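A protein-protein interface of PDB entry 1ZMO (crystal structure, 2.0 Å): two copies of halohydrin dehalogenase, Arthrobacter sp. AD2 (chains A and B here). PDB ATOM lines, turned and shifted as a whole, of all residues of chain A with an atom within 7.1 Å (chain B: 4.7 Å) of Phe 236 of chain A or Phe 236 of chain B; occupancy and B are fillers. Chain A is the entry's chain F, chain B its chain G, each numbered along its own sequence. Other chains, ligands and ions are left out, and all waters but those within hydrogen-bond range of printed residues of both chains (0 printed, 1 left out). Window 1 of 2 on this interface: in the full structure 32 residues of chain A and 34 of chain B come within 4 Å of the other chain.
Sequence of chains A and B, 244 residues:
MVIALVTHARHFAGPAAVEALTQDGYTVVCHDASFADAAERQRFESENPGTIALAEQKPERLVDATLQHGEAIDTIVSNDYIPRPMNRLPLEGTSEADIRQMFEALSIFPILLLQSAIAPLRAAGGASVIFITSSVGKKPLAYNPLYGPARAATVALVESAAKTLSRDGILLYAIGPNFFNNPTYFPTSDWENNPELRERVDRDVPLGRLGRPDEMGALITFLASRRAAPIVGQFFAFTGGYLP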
ATOM      1  N   THR A 133     -23.771  18.605  -3.705  1.00  0.00           N
ATOM      2  CA  THR A 133     -23.610  17.779  -4.873  1.00  0.00           C
ATOM      3  C   THR A 133     -24.982  17.518  -5.497  1.00  0.00           C
ATOM      4  O   THR A 133     -25.570  18.425  -6.059  1.00  0.00           O
ATOM      5  CB  THR A 133     -22.876  16.427  -4.533  1.00  0.00           C
ATOM      6  OG1 THR A 133     -23.678  15.628  -3.660  1.00  0.00           O
ATOM      7  CG2 THR A 133     -21.495  16.725  -3.897  1.00  0.00           C
ATOM      8  N   SER A 134     -25.508  16.302  -5.374  1.00  0.00           N
ATOM      9  CA  SER A 134     -26.814  16.014  -5.976  1.00  0.00           C
ATOM     10  C   SER A 134     -27.238  14.581  -5.584  1.00  0.00           C
ATOM     11  O   SER A 134     -26.387  13.748  -5.209  1.00  0.00           O
ATOM     12  CB  SER A 134     -26.673  16.109  -7.499  1.00  0.00           C
ATOM     13  OG  SER A 134     -27.840  15.673  -8.187  1.00  0.00           O
ATOM     14  N   LYS A 138     -25.205   9.676  -5.438  1.00  0.00           N
ATOM     15  CA  LYS A 138     -25.282   8.350  -4.817  1.00  0.00           C
ATOM     16  C   LYS A 138     -26.199   7.356  -5.533  1.00  0.00           C
ATOM     17  O   LYS A 138     -25.965   6.166  -5.442  1.00  0.00           O
ATOM     18  CB  LYS A 138     -25.752   8.508  -3.367  1.00  0.00           C
ATOM     19  CG  LYS A 138     -24.917   7.787  -2.355  1.00  0.00           C
ATOM     20  CD  LYS A 138     -23.874   8.707  -1.794  1.00  0.00           C
ATOM     21  CE  LYS A 138     -23.107   8.068  -0.657  1.00  0.00           C
ATOM     22  NZ  LYS A 138     -22.105   7.007  -0.992  1.00  0.00           N
ATOM     23  N   VAL A 155     -18.747  13.150  -4.164  1.00  0.00           N
ATOM     24  CA  VAL A 155     -19.254  12.520  -2.924  1.00  0.00           C
ATOM     25  C   VAL A 155     -18.071  11.598  -2.457  1.00  0.00           C
ATOM     26  O   VAL A 155     -17.710  11.552  -1.292  1.00  0.00           O
ATOM     27  CB  VAL A 155     -20.584  11.681  -3.149  1.00  0.00           C
ATOM     28  CG1 VAL A 155     -20.951  10.942  -1.913  1.00  0.00           C
ATOM     29  CG2 VAL A 155     -21.737  12.540  -3.540  1.00  0.00           C
ATOM     30  N   LEU A 172     -15.760  17.334   6.768  1.00  0.00           N
ATOM     31  CA  LEU A 172     -16.397  17.335   5.458  1.00  0.00           C
ATOM     32  C   LEU A 172     -17.753  16.631   5.389  1.00  0.00           C
ATOM     33  O   LEU A 172     -17.932  15.542   5.922  1.00  0.00           O
ATOM     34  CB  LEU A 172     -15.495  16.688   4.405  1.00  0.00           C
ATOM     35  CG  LEU A 172     -14.276  17.438   3.911  1.00  0.00           C
ATOM     36  CD1 LEU A 172     -13.523  18.100   5.008  1.00  0.00           C
ATOM     37  CD2 LEU A 172     -13.396  16.427   3.152  1.00  0.00           C
ATOM     38  N   TYR A 173     -18.683  17.260   4.675  1.00  0.00           N
ATOM     39  CA  TYR A 173     -20.022  16.729   4.456  1.00  0.00           C
ATOM     40  C   TYR A 173     -20.397  16.924   3.004  1.00  0.00           C
ATOM     41  O   TYR A 173     -19.765  17.673   2.310  1.00  0.00           O
ATOM     42  CB  TYR A 173     -21.034  17.445   5.334  1.00  0.00           C
ATOM     43  CG  TYR A 173     -20.629  17.497   6.789  1.00  0.00           C
ATOM     44  CD1 TYR A 173     -20.922  16.456   7.671  1.00  0.00           C
ATOM     45  CD2 TYR A 173     -19.975  18.615   7.283  1.00  0.00           C
ATOM     46  CE1 TYR A 173     -20.572  16.572   9.037  1.00  0.00           C
ATOM     47  CE2 TYR A 173     -19.640  18.741   8.578  1.00  0.00           C
ATOM     48  CZ  TYR A 173     -19.933  17.739   9.473  1.00  0.00           C
ATOM     49  OH  TYR A 173     -19.663  17.958  10.814  1.00  0.00           O
ATOM     50  N   ALA A 174     -21.380  16.153   2.542  1.00  0.00           N
ATOM     51  CA  ALA A 174     -21.896  16.251   1.169  1.00  0.00           C
ATOM     52  C   ALA A 174     -23.424  16.273   1.278  1.00  0.00           C
ATOM     53  O   ALA A 174     -24.000  15.461   1.984  1.00  0.00           O
ATOM     54  CB  ALA A 174     -21.460  14.987   0.285  1.00  0.00           C
ATOM     55  N   ILE A 175     -24.079  17.200   0.607  1.00  0.00           N
ATOM     56  CA  ILE A 175     -25.518  17.187   0.637  1.00  0.00           C
ATOM     57  C   ILE A 175     -25.938  16.898  -0.790  1.00  0.00           C
ATOM     58  O   ILE A 175     -25.348  17.431  -1.703  1.00  0.00           O
ATOM     59  CB  ILE A 175     -26.079  18.544   1.059  1.00  0.00           C
ATOM     60  CG1 ILE A 175     -25.698  18.817   2.511  1.00  0.00           C
ATOM     61  CG2 ILE A 175     -27.587  18.569   0.937  1.00  0.00           C
ATOM     62  CD1 ILE A 175     -25.895  20.328   2.908  1.00  0.00           C
ATOM     63  N   GLY A 176     -26.963  16.073  -0.964  1.00  0.00           N
ATOM     64  CA  GLY A 176     -27.376  15.690  -2.311  1.00  0.00           C
ATOM     65  C   GLY A 176     -28.821  16.028  -2.564  1.00  0.00           C
ATOM     66  O   GLY A 176     -29.713  15.214  -2.340  1.00  0.00           O
ATOM     67  N   PRO A 177     -29.086  17.211  -3.078  1.00  0.00           N
ATOM     68  CA  PRO A 177     -30.500  17.486  -3.295  1.00  0.00           C
ATOM     69  C   PRO A 177     -31.102  16.945  -4.560  1.00  0.00           C
ATOM     70  O   PRO A 177     -30.396  16.501  -5.502  1.00  0.00           O
ATOM     71  CB  PRO A 177     -30.543  19.022  -3.320  1.00  0.00           C
ATOM     72  CG  PRO A 177     -29.173  19.387  -3.899  1.00  0.00           C
ATOM     73  CD  PRO A 177     -28.238  18.396  -3.326  1.00  0.00           C
ATOM     74  N   LEU A 219     -30.050  22.884   7.443  1.00  0.00           N
ATOM     75  CA  LEU A 219     -29.106  21.810   7.436  1.00  0.00           C
ATOM     76  C   LEU A 219     -27.698  22.387   7.379  1.00  0.00           C
ATOM     77  O   LEU A 219     -26.793  21.986   8.125  1.00  0.00           O
ATOM     78  CB  LEU A 219     -29.383  20.965   6.210  1.00  0.00           C
ATOM     79  CG  LEU A 219     -28.376  19.832   5.962  1.00  0.00           C
ATOM     80  CD1 LEU A 219     -28.291  18.966   7.166  1.00  0.00           C
ATOM     81  CD2 LEU A 219     -28.794  19.036   4.772  1.00  0.00           C
ATOM     82  N   LEU A 223     -24.821  21.854  10.226  1.00  0.00           N
ATOM     83  CA  LEU A 223     -23.490  21.270  10.036  1.00  0.00           C
ATOM     84  C   LEU A 223     -22.414  22.277  10.472  1.00  0.00           C
ATOM     85  O   LEU A 223     -21.525  21.964  11.288  1.00  0.00           O
ATOM     86  CB  LEU A 223     -23.289  20.821   8.554  1.00  0.00           C
ATOM     87  CG  LEU A 223     -24.265  19.722   8.079  1.00  0.00           C
ATOM     88  CD1 LEU A 223     -24.043  19.310   6.616  1.00  0.00           C
ATOM     89  CD2 LEU A 223     -24.073  18.531   9.020  1.00  0.00           C
ATOM     90  N   ILE A 231     -21.216  12.968  12.835  1.00  0.00           N
ATOM     91  CA  ILE A 231     -21.816  12.614  11.529  1.00  0.00           C
ATOM     92  C   ILE A 231     -20.960  13.032  10.322  1.00  0.00           C
ATOM     93  O   ILE A 231     -21.427  12.982   9.208  1.00  0.00           O
ATOM     94  CB  ILE A 231     -23.217  13.246  11.312  1.00  0.00           C
ATOM     95  CG1 ILE A 231     -23.102  14.780  11.236  1.00  0.00           C
ATOM     96  CG2 ILE A 231     -24.138  12.779  12.386  1.00  0.00           C
ATOM     97  CD1 ILE A 231     -24.475  15.412  11.207  1.00  0.00           C
ATOM     98  N   VAL A 232     -19.716  13.432  10.579  1.00  0.00           N
ATOM     99  CA  VAL A 232     -18.745  13.847   9.568  1.00  0.00           C
ATOM    100  C   VAL A 232     -18.462  12.785   8.474  1.00  0.00           C
ATOM    101  O   VAL A 232     -18.495  11.578   8.745  1.00  0.00           O
ATOM    102  CB  VAL A 232     -17.431  14.205  10.302  1.00  0.00           C
ATOM    103  CG1 VAL A 232     -16.920  12.959  11.040  1.00  0.00           C
ATOM    104  CG2 VAL A 232     -16.345  14.811   9.360  1.00  0.00           C
ATOM    105  N   GLY A 233     -18.171  13.245   7.257  1.00  0.00           N
ATOM    106  CA  GLY A 233     -17.790  12.360   6.159  1.00  0.00           C
ATOM    107  C   GLY A 233     -18.802  11.451   5.492  1.00  0.00           C
ATOM    108  O   GLY A 233     -18.429  10.473   4.900  1.00  0.00           O
ATOM    109  N   GLN A 234     -20.064  11.836   5.562  1.00  0.00           N
ATOM    110  CA  GLN A 234     -21.246  11.148   5.068  1.00  0.00           C
ATOM    111  C   GLN A 234     -21.941  12.005   4.004  1.00  0.00           C
ATOM    112  O   GLN A 234     -21.773  13.206   3.979  1.00  0.00           O
ATOM    113  CB  GLN A 234     -22.209  11.105   6.227  1.00  0.00           C
ATOM    114  CG  GLN A 234     -22.992   9.880   6.393  1.00  0.00           C
ATOM    115  CD  GLN A 234     -23.843  10.026   7.604  1.00  0.00           C
ATOM    116  OE1 GLN A 234     -23.373  10.526   8.639  1.00  0.00           O
ATOM    117  NE2 GLN A 234     -25.095   9.606   7.510  1.00  0.00           N
ATOM    118  N   PHE A 235     -22.798  11.377   3.209  1.00  0.00           N
ATOM    119  CA  PHE A 235     -23.594  12.063   2.183  1.00  0.00           C
ATOM    120  C   PHE A 235     -25.021  12.182   2.786  1.00  0.00           C
ATOM    121  O   PHE A 235     -25.502  11.210   3.295  1.00  0.00           O
ATOM    122  CB  PHE A 235     -23.625  11.185   0.899  1.00  0.00           C
ATOM    123  CG  PHE A 235     -24.703  11.576  -0.136  1.00  0.00           C
ATOM    124  CD1 PHE A 235     -24.403  12.435  -1.199  1.00  0.00           C
ATOM    125  CD2 PHE A 235     -25.979  11.038  -0.072  1.00  0.00           C
ATOM    126  CE1 PHE A 235     -25.369  12.728  -2.195  1.00  0.00           C
ATOM    127  CE2 PHE A 235     -26.963  11.327  -1.064  1.00  0.00           C
ATOM    128  CZ  PHE A 235     -26.644  12.172  -2.128  1.00  0.00           C
ATOM    129  N   PHE A 236     -25.658  13.354   2.734  1.00  0.00           N
ATOM    130  CA  PHE A 236     -27.025  13.527   3.232  1.00  0.00           C
ATOM    131  C   PHE A 236     -27.966  13.808   2.069  1.00  0.00           C
ATOM    132  O   PHE A 236     -27.879  14.871   1.402  1.00  0.00           O
ATOM    133  CB  PHE A 236     -27.181  14.720   4.254  1.00  0.00           C
ATOM    134  CG  PHE A 236     -26.296  14.595   5.474  1.00  0.00           C
ATOM    135  CD1 PHE A 236     -25.214  15.458   5.657  1.00  0.00           C
ATOM    136  CD2 PHE A 236     -26.461  13.531   6.377  1.00  0.00           C
ATOM    137  CE1 PHE A 236     -24.300  15.255   6.717  1.00  0.00           C
ATOM    138  CE2 PHE A 236     -25.547  13.317   7.439  1.00  0.00           C
ATOM    139  CZ  PHE A 236     -24.466  14.176   7.612  1.00  0.00           C
ATOM    140  N   ALA A 237     -28.854  12.853   1.816  1.00  0.00           N
ATOM    141  CA  ALA A 237     -29.878  13.022   0.797  1.00  0.00           C
ATOM    142  C   ALA A 237     -30.754  14.211   1.254  1.00  0.00           C
ATOM    143  O   ALA A 237     -30.934  14.420   2.455  1.00  0.00           O
ATOM    144  CB  ALA A 237     -30.672  11.781   0.730  1.00  0.00           C
ATOM    145  N   PHE A 238     -31.263  15.015   0.314  1.00  0.00           N
ATOM    146  CA  PHE A 238     -32.117  16.192   0.664  1.00  0.00           C
ATOM    147  C   PHE A 238     -33.095  16.142  -0.502  1.00  0.00           C
ATOM    148  O   PHE A 238     -33.036  16.964  -1.448  1.00  0.00           O
ATOM    149  CB  PHE A 238     -31.288  17.512   0.665  1.00  0.00           C
ATOM    150  CG  PHE A 238     -32.055  18.743   1.125  1.00  0.00           C
ATOM    151  CD1 PHE A 238     -32.083  19.119   2.486  1.00  0.00           C
ATOM    152  CD2 PHE A 238     -32.799  19.487   0.214  1.00  0.00           C
ATOM    153  CE1 PHE A 238     -32.837  20.201   2.913  1.00  0.00           C
ATOM    154  CE2 PHE A 238     -33.568  20.584   0.652  1.00  0.00           C
ATOM    155  CZ  PHE A 238     -33.583  20.930   1.989  1.00  0.00           C
ATOM    156  N   THR A 239     -33.998  15.157  -0.417  1.00  0.00           N
ATOM    157  CA  THR A 239     -34.902  14.916  -1.515  1.00  0.00           C
ATOM    158  C   THR A 239     -36.355  14.780  -1.165  1.00  0.00           C
ATOM    159  O   THR A 239     -37.144  14.473  -2.020  1.00  0.00           O
ATOM    160  CB  THR A 239     -34.439  13.621  -2.271  1.00  0.00           C
ATOM    161  OG1 THR A 239     -34.606  12.468  -1.431  1.00  0.00           O
ATOM    162  CG2 THR A 239     -32.957  13.739  -2.651  1.00  0.00           C
ATOM    163  N   LEU A 243     -35.016   9.604  -2.111  1.00  0.00           N
ATOM    164  CA  LEU A 243     -33.960   8.611  -1.782  1.00  0.00           C
ATOM    165  C   LEU A 243     -34.260   8.192  -0.330  1.00  0.00           C
ATOM    166  O   LEU A 243     -34.839   8.964   0.424  1.00  0.00           O
ATOM    167  CB  LEU A 243     -32.560   9.265  -1.818  1.00  0.00           C
ATOM    168  CG  LEU A 243     -32.087   9.840  -3.160  1.00  0.00           C
ATOM    169  CD1 LEU A 243     -30.588  10.252  -3.057  1.00  0.00           C
ATOM    170  CD2 LEU A 243     -32.284   8.836  -4.225  1.00  0.00           C
ATOM    171  N   TYR B 173     -36.667   8.726  10.792  1.00  0.00           N
ATOM    172  CA  TYR B 173     -35.219   8.753  10.584  1.00  0.00           C
ATOM    173  C   TYR B 173     -34.604   7.591  11.333  1.00  0.00           C
ATOM    174  O   TYR B 173     -35.236   7.040  12.224  1.00  0.00           O
ATOM    175  CB  TYR B 173     -34.580  10.021  11.149  1.00  0.00           C
ATOM    176  CG  TYR B 173     -35.234  11.326  10.710  1.00  0.00           C
ATOM    177  CD1 TYR B 173     -34.878  11.938   9.512  1.00  0.00           C
ATOM    178  CD2 TYR B 173     -36.213  11.940  11.510  1.00  0.00           C
ATOM    179  CE1 TYR B 173     -35.464  13.123   9.113  1.00  0.00           C
ATOM    180  CE2 TYR B 173     -36.811  13.117  11.135  1.00  0.00           C
ATOM    181  CZ  TYR B 173     -36.439  13.708   9.925  1.00  0.00           C
ATOM    182  OH  TYR B 173     -37.085  14.815   9.486  1.00  0.00           O
ATOM    183  N   ALA B 174     -33.381   7.240  10.936  1.00  0.00           N
ATOM    184  CA  ALA B 174     -32.580   6.227  11.617  1.00  0.00           C
ATOM    185  C   ALA B 174     -31.204   6.836  11.822  1.00  0.00           C
ATOM    186  O   ALA B 174     -30.632   7.477  10.913  1.00  0.00           O
ATOM    187  CB  ALA B 174     -32.447   4.938  10.795  1.00  0.00           C
ATOM    188  N   ILE B 175     -30.681   6.655  13.030  1.00  0.00           N
ATOM    189  CA  ILE B 175     -29.346   7.093  13.376  1.00  0.00           C
ATOM    190  C   ILE B 175     -28.635   5.760  13.731  1.00  0.00           C
ATOM    191  O   ILE B 175     -29.171   4.953  14.518  1.00  0.00           O
ATOM    192  CB  ILE B 175     -29.387   8.035  14.642  1.00  0.00           C
ATOM    193  CG1 ILE B 175     -30.262   9.272  14.378  1.00  0.00           C
ATOM    194  CG2 ILE B 175     -27.982   8.512  14.975  1.00  0.00           C
ATOM    195  CD1 ILE B 175     -30.472  10.200  15.659  1.00  0.00           C
ATOM    196  N   GLY B 176     -27.471   5.499  13.146  1.00  0.00           N
ATOM    197  CA  GLY B 176     -26.766   4.250  13.445  1.00  0.00           C
ATOM    198  C   GLY B 176     -25.437   4.618  14.048  1.00  0.00           C
ATOM    199  O   GLY B 176     -24.471   4.855  13.327  1.00  0.00           O
ATOM    200  N   LEU B 223     -33.225  17.000  14.546  1.00  0.00           N
ATOM    201  CA  LEU B 223     -34.261  16.293  13.776  1.00  0.00           C
ATOM    202  C   LEU B 223     -35.671  16.640  14.298  1.00  0.00           C
ATOM    203  O   LEU B 223     -36.578  16.937  13.488  1.00  0.00           O
ATOM    204  CB  LEU B 223     -33.979  14.805  13.780  1.00  0.00           C
ATOM    205  CG  LEU B 223     -32.699  14.321  12.970  1.00  0.00           C
ATOM    206  CD1 LEU B 223     -32.466  12.830  13.201  1.00  0.00           C
ATOM    207  CD2 LEU B 223     -32.835  14.534  11.452  1.00  0.00           C
ATOM    208  N   ILE B 231     -34.680  15.909   4.580  1.00  0.00           N
ATOM    209  CA  ILE B 231     -33.724  14.798   4.775  1.00  0.00           C
ATOM    210  C   ILE B 231     -34.441  13.597   5.438  1.00  0.00           C
ATOM    211  O   ILE B 231     -33.831  12.703   5.985  1.00  0.00           O
ATOM    212  CB  ILE B 231     -32.469  15.217   5.648  1.00  0.00           C
ATOM    213  CG1 ILE B 231     -32.909  15.587   7.076  1.00  0.00           C
ATOM    214  CG2 ILE B 231     -31.728  16.395   4.983  1.00  0.00           C
ATOM    215  CD1 ILE B 231     -31.798  16.143   7.933  1.00  0.00           C
ATOM    216  N   GLN B 234     -33.987   8.734   5.846  1.00  0.00           N
ATOM    217  CA  GLN B 234     -32.723   8.085   5.674  1.00  0.00           C
ATOM    218  C   GLN B 234     -32.013   7.739   6.961  1.00  0.00           C
ATOM    219  O   GLN B 234     -32.426   8.100   8.047  1.00  0.00           O
ATOM    220  CB  GLN B 234     -31.812   8.946   4.823  1.00  0.00           C
ATOM    221  CG  GLN B 234     -31.494  10.287   5.452  1.00  0.00           C
ATOM    222  CD  GLN B 234     -30.645  11.141   4.504  1.00  0.00           C
ATOM    223  OE1 GLN B 234     -29.626  10.679   3.976  1.00  0.00           O
ATOM    224  NE2 GLN B 234     -31.060  12.392   4.296  1.00  0.00           N
ATOM    225  N   PHE B 235     -30.876   7.074   6.783  1.00  0.00           N
ATOM    226  CA  PHE B 235     -30.006   6.629   7.865  1.00  0.00           C
ATOM    227  C   PHE B 235     -28.837   7.603   7.955  1.00  0.00           C
ATOM    228  O   PHE B 235     -28.251   7.945   6.960  1.00  0.00           O
ATOM    229  CB  PHE B 235     -29.526   5.201   7.514  1.00  0.00           C
ATOM    230  CG  PHE B 235     -28.437   4.627   8.408  1.00  0.00           C
ATOM    231  CD1 PHE B 235     -28.753   3.721   9.429  1.00  0.00           C
ATOM    232  CD2 PHE B 235     -27.093   4.850   8.126  1.00  0.00           C
ATOM    233  CE1 PHE B 235     -27.754   3.043  10.144  1.00  0.00           C
ATOM    234  CE2 PHE B 235     -26.095   4.191   8.832  1.00  0.00           C
ATOM    235  CZ  PHE B 235     -26.430   3.279   9.846  1.00  0.00           C
ATOM    236  N   PHE B 236     -28.523   8.037   9.162  1.00  0.00           N
ATOM    237  CA  PHE B 236     -27.408   8.921   9.401  1.00  0.00           C
ATOM    238  C   PHE B 236     -26.376   8.153  10.234  1.00  0.00           C
ATOM    239  O   PHE B 236     -26.674   7.674  11.336  1.00  0.00           O
ATOM    240  CB  PHE B 236     -27.852  10.188  10.155  1.00  0.00           C
ATOM    241  CG  PHE B 236     -28.995  10.902   9.505  1.00  0.00           C
ATOM    242  CD1 PHE B 236     -30.299  10.672   9.925  1.00  0.00           C
ATOM    243  CD2 PHE B 236     -28.781  11.793   8.451  1.00  0.00           C
ATOM    244  CE1 PHE B 236     -31.375  11.326   9.289  1.00  0.00           C
ATOM    245  CE2 PHE B 236     -29.864  12.460   7.811  1.00  0.00           C
ATOM    246  CZ  PHE B 236     -31.138  12.228   8.219  1.00  0.00           C
ATOM    247  N   ALA B 237     -25.174   7.987   9.687  1.00  0.00           N
ATOM    248  CA  ALA B 237     -24.107   7.325  10.424  1.00  0.00           C
ATOM    249  C   ALA B 237     -23.691   8.282  11.551  1.00  0.00           C
ATOM    250  O   ALA B 237     -23.595   9.479  11.309  1.00  0.00           O
ATOM    251  CB  ALA B 237     -22.897   7.072   9.503  1.00  0.00           C
ATOM    252  N   PHE B 238     -23.396   7.758  12.749  1.00  0.00           N
ATOM    253  CA  PHE B 238     -22.946   8.587  13.910  1.00  0.00           C
ATOM    254  C   PHE B 238     -21.737   7.846  14.450  1.00  0.00           C
ATOM    255  O   PHE B 238     -21.773   7.328  15.550  1.00  0.00           O
ATOM    256  CB  PHE B 238     -24.035   8.689  15.009  1.00  0.00           C
ATOM    257  CG  PHE B 238     -23.724   9.723  16.114  1.00  0.00           C
ATOM    258  CD1 PHE B 238     -24.088  11.047  15.981  1.00  0.00           C
ATOM    259  CD2 PHE B 238     -23.016   9.349  17.267  1.00  0.00           C
ATOM    260  CE1 PHE B 238     -23.749  11.986  16.973  1.00  0.00           C
ATOM    261  CE2 PHE B 238     -22.667  10.252  18.238  1.00  0.00           C
ATOM    262  CZ  PHE B 238     -23.035  11.584  18.096  1.00  0.00           C
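Ile 231 of chain A touches Ala 237 of chain B, and with the chains exchanged Ala 237 of chain A touches Ile 231 of chain B. Gln 234 of chain A touches Phe 235 of chain B, but with the chains exchanged Phe 235 of chain A does not touch Gln 234 of chain B (4.2 Å). Gln 234 of chain A touches Phe 236 of chain B, and with the chains exchanged Phe 236 of chain A touches Gln 234 of chain B. Phe 236 of chain B touches its own counterpart, Phe 236 of chain A. Of the 11 pairs that touch across the chains among the printed residues, 9 have their exchanged pair printed and touching as well.
Of chain B, only Gln 234 (3.9 Å) and Phe 236 (3.6 Å) come within 4 Å of Phe 236 of chain A. Of the printed residues of chain A, Phe 236 of chain B touches Gln 234 and Phe 236. Of the printed residues of chain A, Ala 237 of chain B touches Ile 231 (3.5 Å) and Gln 234 (2.7 Å). Of the printed residues of chain A, Phe 235 of chain B touches Gln 234. Of the printed residues of chain A, Phe 238 of chain B touches Ile 231. Leu 243 of chain A touches none of the printed residues of chain B. Ile 175 of chain B touches none of the printed residues of chain A. The nearest printed residue of chain B that does not touch Phe 236 of chain A is Ile 231 of chain B (4.9 Å). The nearest printed residue of chain A that does not touch Gln 234 of chain B is Phe 235 of chain A (4.2 Å).
N of Ala 237 of chain B sits close to NE2 of Gln 234 of chain A (2.7 Å). The side-chain amide nitrogen (NE2) of Gln 234 of chain B sits at hydrogen-bond distance from the backbone carbonyl oxygen (O) of Ala 237 of chain A.
O of Gln 234 of chain A sits at hydrogen-bond distance from N of Ala 174 of chain A (3.3 Å). The backbone carbonyl oxygen (O) of Ile 231 of chain A lies close to the side-chain amide oxygen (OE1) of Gln 234 of chain A (3.2 Å). The backbone carbonyl oxygen of Gly 176 of chain A lies within hydrogen-bond range of the backbone NH of Phe 238 of chain A (3.1 Å). N of Ala 174 of chain B sits at hydrogen-bond distance from O of Gln 234 of chain B. The side-chain amide nitrogen of Gln 234 of chain B lies within hydrogen-bond range of the backbone carbonyl oxygen of Ile 231 of chain B (3.3 Å). The backbone carbonyl oxygen of Phe 236 of chain B sits at hydrogen-bond distance from the backbone NH of Gly 176 of chain B.
Hydrophobic or aromatic side chains of chain A within 4 Å of the printed part of chain B: Leu 219, Ile 231, Phe 236, Ala 237 and Phe 238. Among the printed residues, 11 pairs touch across the chains.
Among the printed residues, pairs that only touch across the chains: Gln 234 of chain A with Phe 236 of chain B (3.1 Å), Ala 237 of chain A with Ile 231 of chain B (3.3 Å), Ile 231 of chain A with Ala 237 of chain B (3.5 Å), Phe 236 of chain A with Phe 236 of chain B (3.6 Å), Gln 234 of chain A with Phe 235 of chain B (3.6 Å), Phe 238 of chain A with Ile 231 of chain B (3.7 Å), Phe 236 of chain A with Gln 234 of chain B (3.9 Å), Leu 219 of chain A with Ile 231 of chain B (3.95 Å) and Ile 231 of chain A with Phe 238 of chain B (3.99 Å).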
